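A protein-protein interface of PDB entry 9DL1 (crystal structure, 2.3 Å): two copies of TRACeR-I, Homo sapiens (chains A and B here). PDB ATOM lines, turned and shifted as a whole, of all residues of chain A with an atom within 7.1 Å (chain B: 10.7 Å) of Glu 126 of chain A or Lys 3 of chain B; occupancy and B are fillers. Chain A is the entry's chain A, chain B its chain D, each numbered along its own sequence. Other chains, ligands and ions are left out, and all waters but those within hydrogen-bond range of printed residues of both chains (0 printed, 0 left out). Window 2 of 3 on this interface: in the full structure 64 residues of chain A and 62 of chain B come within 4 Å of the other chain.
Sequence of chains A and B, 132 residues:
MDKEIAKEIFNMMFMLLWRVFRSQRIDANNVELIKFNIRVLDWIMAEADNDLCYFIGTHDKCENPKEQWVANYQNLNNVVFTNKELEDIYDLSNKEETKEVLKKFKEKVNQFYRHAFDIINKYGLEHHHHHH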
ATOM      1  N   ILE A 120     -10.174  33.554  -2.732  1.00  0.00           N
ATOM      2  CA  ILE A 120     -11.012  32.488  -2.189  1.00  0.00           C
ATOM      3  C   ILE A 120     -12.279  32.350  -3.024  1.00  0.00           C
ATOM      4  O   ILE A 120     -12.670  31.245  -3.412  1.00  0.00           O
ATOM      5  CB  ILE A 120     -11.342  32.746  -0.705  1.00  0.00           C
ATOM      6  CG1 ILE A 120     -10.124  32.528   0.190  1.00  0.00           C
ATOM      7  CG2 ILE A 120     -12.422  31.802  -0.248  1.00  0.00           C
ATOM      8  CD1 ILE A 120      -9.303  31.249  -0.110  1.00  0.00           C
ATOM      9  N   ASN A 121     -12.930  33.478  -3.329  1.00  0.00           N
ATOM     10  CA  ASN A 121     -14.149  33.453  -4.133  1.00  0.00           C
ATOM     11  C   ASN A 121     -13.912  32.824  -5.504  1.00  0.00           C
ATOM     12  O   ASN A 121     -14.744  32.056  -5.994  1.00  0.00           O
ATOM     13  CB  ASN A 121     -14.689  34.872  -4.310  1.00  0.00           C
ATOM     14  CG  ASN A 121     -15.303  35.444  -3.039  1.00  0.00           C
ATOM     15  OD1 ASN A 121     -15.674  34.712  -2.124  1.00  0.00           O
ATOM     16  ND2 ASN A 121     -15.407  36.779  -2.980  1.00  0.00           N
ATOM     17  N   TYR A 123     -11.307  30.805  -6.689  1.00  0.00           N
ATOM     18  CA  TYR A 123     -10.688  29.489  -6.814  1.00  0.00           C
ATOM     19  C   TYR A 123     -10.801  28.609  -5.580  1.00  0.00           C
ATOM     20  O   TYR A 123     -10.550  27.409  -5.696  1.00  0.00           O
ATOM     21  CB  TYR A 123      -9.196  29.612  -7.162  1.00  0.00           C
ATOM     22  CG  TYR A 123      -8.838  30.606  -8.247  1.00  0.00           C
ATOM     23  CD1 TYR A 123      -8.920  30.261  -9.591  1.00  0.00           C
ATOM     24  CD2 TYR A 123      -8.392  31.882  -7.927  1.00  0.00           C
ATOM     25  CE1 TYR A 123      -8.582  31.169 -10.585  1.00  0.00           C
ATOM     26  CE2 TYR A 123      -8.055  32.794  -8.915  1.00  0.00           C
ATOM     27  CZ  TYR A 123      -8.149  32.427 -10.242  1.00  0.00           C
ATOM     28  OH  TYR A 123      -7.809  33.329 -11.217  1.00  0.00           O
ATOM     29  N   GLY A 124     -11.173  29.150  -4.418  1.00  0.00           N
ATOM     30  CA  GLY A 124     -11.108  28.396  -3.178  1.00  0.00           C
ATOM     31  C   GLY A 124     -12.416  27.765  -2.759  1.00  0.00           C
ATOM     32  O   GLY A 124     -12.440  26.876  -1.909  1.00  0.00           O
ATOM     33  N   LEU A 125     -13.512  28.229  -3.343  1.00  0.00           N
ATOM     34  CA  LEU A 125     -14.829  27.654  -3.121  1.00  0.00           C
ATOM     35  C   LEU A 125     -15.211  26.742  -4.282  1.00  0.00           C
ATOM     36  O   LEU A 125     -14.905  27.034  -5.444  1.00  0.00           O
ATOM     37  CB  LEU A 125     -15.874  28.755  -2.963  1.00  0.00           C
ATOM     38  CG  LEU A 125     -15.653  29.674  -1.766  1.00  0.00           C
ATOM     39  CD1 LEU A 125     -16.522  30.920  -1.896  1.00  0.00           C
ATOM     40  CD2 LEU A 125     -15.909  28.933  -0.459  1.00  0.00           C
ATOM     41  N   GLU A 126     -15.892  25.641  -3.963  1.00  0.00           N
ATOM     42  CA  GLU A 126     -16.372  24.706  -4.973  1.00  0.00           C
ATOM     43  C   GLU A 126     -17.881  24.825  -5.194  1.00  0.00           C
ATOM     44  O   GLU A 126     -18.504  23.888  -5.702  1.00  0.00           O
ATOM     45  CB  GLU A 126     -15.988  23.272  -4.590  1.00  0.00           C
ATOM     46  CG  GLU A 126     -16.661  22.756  -3.307  1.00  0.00           C
ATOM     47  CD  GLU A 126     -16.005  23.262  -2.022  1.00  0.00           C
ATOM     48  OE1 GLU A 126     -16.287  24.427  -1.625  1.00  0.00           O
ATOM     49  OE2 GLU A 126     -15.216  22.492  -1.418  1.00  0.00           O
ATOM     50  N   HIS A 127     -18.478  25.960  -4.829  1.00  0.00           N
ATOM     51  CA  HIS A 127     -19.933  26.149  -4.932  1.00  0.00           C
ATOM     52  C   HIS A 127     -20.312  27.611  -5.209  1.00  0.00           C
ATOM     53  O   HIS A 127     -19.445  28.479  -5.380  1.00  0.00           O
ATOM     54  CB  HIS A 127     -20.627  25.651  -3.651  1.00  0.00           C
ATOM     55  CG  HIS A 127     -19.731  25.615  -2.443  1.00  0.00           C
ATOM     56  ND1 HIS A 127     -19.045  26.720  -1.982  1.00  0.00           N
ATOM     57  CD2 HIS A 127     -19.409  24.602  -1.602  1.00  0.00           C
ATOM     58  CE1 HIS A 127     -18.341  26.391  -0.912  1.00  0.00           C
ATOM     59  NE2 HIS A 127     -18.543  25.112  -0.663  1.00  0.00           N
ATOM     60  N   ASP B   2      -6.935  24.811  -8.445  1.00  0.00           N
ATOM     61  CA  ASP B   2      -6.988  23.973  -7.246  1.00  0.00           C
ATOM     62  C   ASP B   2      -7.370  24.809  -6.014  1.00  0.00           C
ATOM     63  O   ASP B   2      -6.740  25.838  -5.737  1.00  0.00           O
ATOM     64  CB  ASP B   2      -5.643  23.294  -7.032  1.00  0.00           C
ATOM     65  CG  ASP B   2      -5.722  22.069  -6.156  1.00  0.00           C
ATOM     66  OD1 ASP B   2      -6.050  20.959  -6.641  1.00  0.00           O
ATOM     67  OD2 ASP B   2      -5.414  22.209  -4.968  1.00  0.00           O
ATOM     68  N   LYS B   3      -8.405  24.357  -5.288  1.00  0.00           N
ATOM     69  CA  LYS B   3      -8.844  25.056  -4.080  1.00  0.00           C
ATOM     70  C   LYS B   3      -7.739  25.121  -3.035  1.00  0.00           C
ATOM     71  O   LYS B   3      -7.604  26.132  -2.333  1.00  0.00           O
ATOM     72  CB  LYS B   3     -10.075  24.380  -3.467  1.00  0.00           C
ATOM     73  CG  LYS B   3     -10.958  23.661  -4.444  1.00  0.00           C
ATOM     74  CD  LYS B   3     -12.191  23.083  -3.744  1.00  0.00           C
ATOM     75  CE  LYS B   3     -12.499  21.680  -4.266  1.00  0.00           C
ATOM     76  NZ  LYS B   3     -13.660  21.066  -3.564  1.00  0.00           N
ATOM     77  N   GLU B   4      -6.955  24.043  -2.903  1.00  0.00           N
ATOM     78  CA  GLU B   4      -5.897  24.019  -1.897  1.00  0.00           C
ATOM     79  C   GLU B   4      -4.848  25.081  -2.170  1.00  0.00           C
ATOM     80  O   GLU B   4      -4.448  25.811  -1.255  1.00  0.00           O
ATOM     81  CB  GLU B   4      -5.246  22.642  -1.831  1.00  0.00           C
ATOM     82  CG  GLU B   4      -6.092  21.649  -1.081  1.00  0.00           C
ATOM     83  CD  GLU B   4      -6.721  22.257   0.160  1.00  0.00           C
ATOM     84  OE1 GLU B   4      -5.974  22.849   0.979  1.00  0.00           O
ATOM     85  OE2 GLU B   4      -7.961  22.154   0.308  1.00  0.00           O
ATOM     86  N   ILE B   5      -4.393  25.181  -3.424  1.00  0.00           N
ATOM     87  CA  ILE B   5      -3.405  26.190  -3.782  1.00  0.00           C
ATOM     88  C   ILE B   5      -3.933  27.581  -3.471  1.00  0.00           C
ATOM     89  O   ILE B   5      -3.231  28.414  -2.889  1.00  0.00           O
ATOM     90  CB  ILE B   5      -3.015  26.067  -5.267  1.00  0.00           C
ATOM     91  CG1 ILE B   5      -2.452  24.675  -5.560  1.00  0.00           C
ATOM     92  CG2 ILE B   5      -1.997  27.141  -5.608  1.00  0.00           C
ATOM     93  CD1 ILE B   5      -2.286  24.359  -7.033  1.00  0.00           C
ATOM     94  N   ALA B   6      -5.175  27.856  -3.873  1.00  0.00           N
ATOM     95  CA  ALA B   6      -5.775  29.150  -3.568  1.00  0.00           C
ATOM     96  C   ALA B   6      -5.822  29.390  -2.060  1.00  0.00           C
ATOM     97  O   ALA B   6      -5.490  30.483  -1.586  1.00  0.00           O
ATOM     98  CB  ALA B   6      -7.174  29.245  -4.188  1.00  0.00           C
ATOM     99  N   LYS B   7      -6.189  28.368  -1.290  1.00  0.00           N
ATOM    100  CA  LYS B   7      -6.273  28.550   0.151  1.00  0.00           C
ATOM    101  C   LYS B   7      -4.907  28.867   0.735  1.00  0.00           C
ATOM    102  O   LYS B   7      -4.784  29.721   1.620  1.00  0.00           O
ATOM    103  CB  LYS B   7      -6.888  27.304   0.788  1.00  0.00           C
ATOM    104  CG  LYS B   7      -8.412  27.304   0.627  1.00  0.00           C
ATOM    105  CD  LYS B   7      -8.998  25.933   0.631  1.00  0.00           C
ATOM    106  CE  LYS B   7      -8.855  25.307   1.993  1.00  0.00           C
ATOM    107  NZ  LYS B   7      -9.566  24.018   2.029  1.00  0.00           N
ATOM    108  N   GLU B   8      -3.863  28.223   0.210  1.00  0.00           N
ATOM    109  CA  GLU B   8      -2.511  28.416   0.725  1.00  0.00           C
ATOM    110  C   GLU B   8      -1.983  29.808   0.417  1.00  0.00           C
ATOM    111  O   GLU B   8      -1.209  30.365   1.210  1.00  0.00           O
ATOM    112  CB  GLU B   8      -1.573  27.365   0.129  1.00  0.00           C
ATOM    113  CG  GLU B   8      -1.741  25.967   0.721  1.00  0.00           C
ATOM    114  CD  GLU B   8      -1.163  24.868  -0.174  1.00  0.00           C
ATOM    115  OE1 GLU B   8      -0.600  25.205  -1.243  1.00  0.00           O
ATOM    116  OE2 GLU B   8      -1.260  23.671   0.202  1.00  0.00           O
ATOM    117  N   ILE B   9      -2.379  30.365  -0.735  1.00  0.00           N
ATOM    118  CA  ILE B   9      -1.966  31.702  -1.121  1.00  0.00           C
ATOM    119  C   ILE B   9      -2.688  32.735  -0.273  1.00  0.00           C
ATOM    120  O   ILE B   9      -2.073  33.673   0.243  1.00  0.00           O
ATOM    121  CB  ILE B   9      -2.205  31.899  -2.631  1.00  0.00           C
ATOM    122  CG1 ILE B   9      -1.212  31.045  -3.422  1.00  0.00           C
ATOM    123  CG2 ILE B   9      -2.104  33.361  -3.036  1.00  0.00           C
ATOM    124  CD1 ILE B   9      -1.645  30.805  -4.886  1.00  0.00           C
ATOM    125  N   PHE B  10      -3.995  32.560  -0.085  1.00  0.00           N
ATOM    126  CA  PHE B  10      -4.726  33.388   0.868  1.00  0.00           C
ATOM    127  C   PHE B  10      -4.060  33.354   2.244  1.00  0.00           C
ATOM    128  O   PHE B  10      -3.815  34.398   2.859  1.00  0.00           O
ATOM    129  CB  PHE B  10      -6.183  32.905   0.933  1.00  0.00           C
ATOM    130  CG  PHE B  10      -7.005  33.576   1.986  1.00  0.00           C
ATOM    131  CD1 PHE B  10      -6.974  33.120   3.311  1.00  0.00           C
ATOM    132  CD2 PHE B  10      -7.810  34.673   1.665  1.00  0.00           C
ATOM    133  CE1 PHE B  10      -7.735  33.742   4.298  1.00  0.00           C
ATOM    134  CE2 PHE B  10      -8.589  35.296   2.647  1.00  0.00           C
ATOM    135  CZ  PHE B  10      -8.550  34.829   3.968  1.00  0.00           C
ATOM    136  N   ASN B  11      -3.754  32.152   2.736  1.00  0.00           N
ATOM    137  CA  ASN B  11      -3.207  32.011   4.080  1.00  0.00           C
ATOM    138  C   ASN B  11      -1.855  32.702   4.198  1.00  0.00           C
ATOM    139  O   ASN B  11      -1.584  33.404   5.181  1.00  0.00           O
ATOM    140  CB  ASN B  11      -3.079  30.528   4.445  1.00  0.00           C
ATOM    141  CG  ASN B  11      -2.631  30.320   5.904  1.00  0.00           C
ATOM    142  OD1 ASN B  11      -3.337  30.696   6.856  1.00  0.00           O
ATOM    143  ND2 ASN B  11      -1.453  29.719   6.079  1.00  0.00           N
ATOM    144  N   LEU B  52      -0.685  32.658  -8.361  1.00  0.00           N
ATOM    145  CA  LEU B  52      -1.919  32.220  -9.008  1.00  0.00           C
ATOM    146  C   LEU B  52      -1.685  31.898 -10.474  1.00  0.00           C
ATOM    147  O   LEU B  52      -2.253  30.939 -11.003  1.00  0.00           O
ATOM    148  CB  LEU B  52      -2.986  33.303  -8.910  1.00  0.00           C
ATOM    149  CG  LEU B  52      -3.711  33.594  -7.602  1.00  0.00           C
ATOM    150  CD1 LEU B  52      -4.591  34.820  -7.831  1.00  0.00           C
ATOM    151  CD2 LEU B  52      -4.529  32.385  -7.156  1.00  0.00           C
ATOM    152  N   PHE B  55       0.816  28.504 -10.750  1.00  0.00           N
ATOM    153  CA  PHE B  55       0.068  27.332 -10.311  1.00  0.00           C
ATOM    154  C   PHE B  55      -1.393  27.500 -10.758  1.00  0.00           C
ATOM    155  O   PHE B  55      -1.679  28.297 -11.656  1.00  0.00           O
ATOM    156  CB  PHE B  55       0.211  27.166  -8.790  1.00  0.00           C
ATOM    157  CG  PHE B  55       1.639  27.310  -8.257  1.00  0.00           C
ATOM    158  CD1 PHE B  55       2.516  26.235  -8.276  1.00  0.00           C
ATOM    159  CD2 PHE B  55       2.076  28.506  -7.685  1.00  0.00           C
ATOM    160  CE1 PHE B  55       3.811  26.356  -7.770  1.00  0.00           C
ATOM    161  CE2 PHE B  55       3.359  28.633  -7.177  1.00  0.00           C
ATOM    162  CZ  PHE B  55       4.235  27.554  -7.226  1.00  0.00           C
ATOM    163  N   ILE B  56      -2.325  26.770 -10.138  1.00  0.00           N
ATOM    164  CA  ILE B  56      -3.768  26.971 -10.344  1.00  0.00           C
ATOM    165  C   ILE B  56      -4.105  27.036 -11.827  1.00  0.00           C
ATOM    166  O   ILE B  56      -4.335  28.127 -12.368  1.00  0.00           O
ATOM    167  CB  ILE B  56      -4.292  28.247  -9.649  1.00  0.00           C
ATOM    168  CG1 ILE B  56      -4.194  28.115  -8.132  1.00  0.00           C
ATOM    169  CG2 ILE B  56      -5.756  28.500 -10.011  1.00  0.00           C
ATOM    170  CD1 ILE B  56      -5.217  28.941  -7.364  1.00  0.00           C
ATOM    171  N   GLY B  57      -4.155  25.876 -12.490  1.00  0.00           N
ATOM    172  CA  GLY B  57      -4.281  25.858 -13.934  1.00  0.00           C
ATOM    173  C   GLY B  57      -3.336  26.883 -14.531  1.00  0.00           C
ATOM    174  O   GLY B  57      -2.182  26.565 -14.851  1.00  0.00           O
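CG1 of Ile 120 of chain A touches CD2 of Phe 10 of chain B, 3.5 Å away.
Lys 3 of chain B touches Tyr 123 of chain A (CA to O, 3.3 Å).
Tyr 123 of chain A touches Ala 6 of chain B.
Tyr 123 of chain A touches Leu 52 of chain B.
CG2 of Ile 56 of chain B touches CD1 of Tyr 123 of chain A (3.6 Å).
Gly 124 of chain A touches Lys 3 of chain B.
Of chain B, only Lys 3 comes within 4 Å of Glu 126 of chain A.
Lys 3 of chain B touches just these residues of chain A: Tyr 123, Gly 124 and Glu 126.
No residue of chain B comes within 4 Å of Leu 125 of chain A.
No residue of chain B comes within 4 Å of His 127 of chain A.
Printed residues of chain B within 4 Å of Gly 124 of chain A: Lys 3 (3.8 Å).
Of the printed residues of chain A, Phe 10 of chain B touches Ile 120.
Asn 11 of chain B touches none of the printed residues of chain A.
The nearest residue of chain B that does not touch Glu 126 of chain A is Lys 7 of chain B (6.8 Å).
The nearest residue of chain A that does not touch Lys 3 of chain B is Leu 125 of chain A (4.8 Å).
Of the 14 printed residues of chain B, 5 touch a printed residue of chain A.
Among the printed residues, 7 pairs touch across the chains.
O of Ile 120 of chain A is in hydrogen-bond range of N of Leu 125 of chain A, 3.1 Å away.
NE2 of His 127 of chain A lies within hydrogen-bond range of OE1 of Glu 126 of chain A, at 2.5 Å.
The side-chain carboxylate of Glu 126 of chain A is in salt-bridge range of the side-chain amino group of Lys 3 of chain B (3.0 Å).
No position is printed for both chains.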
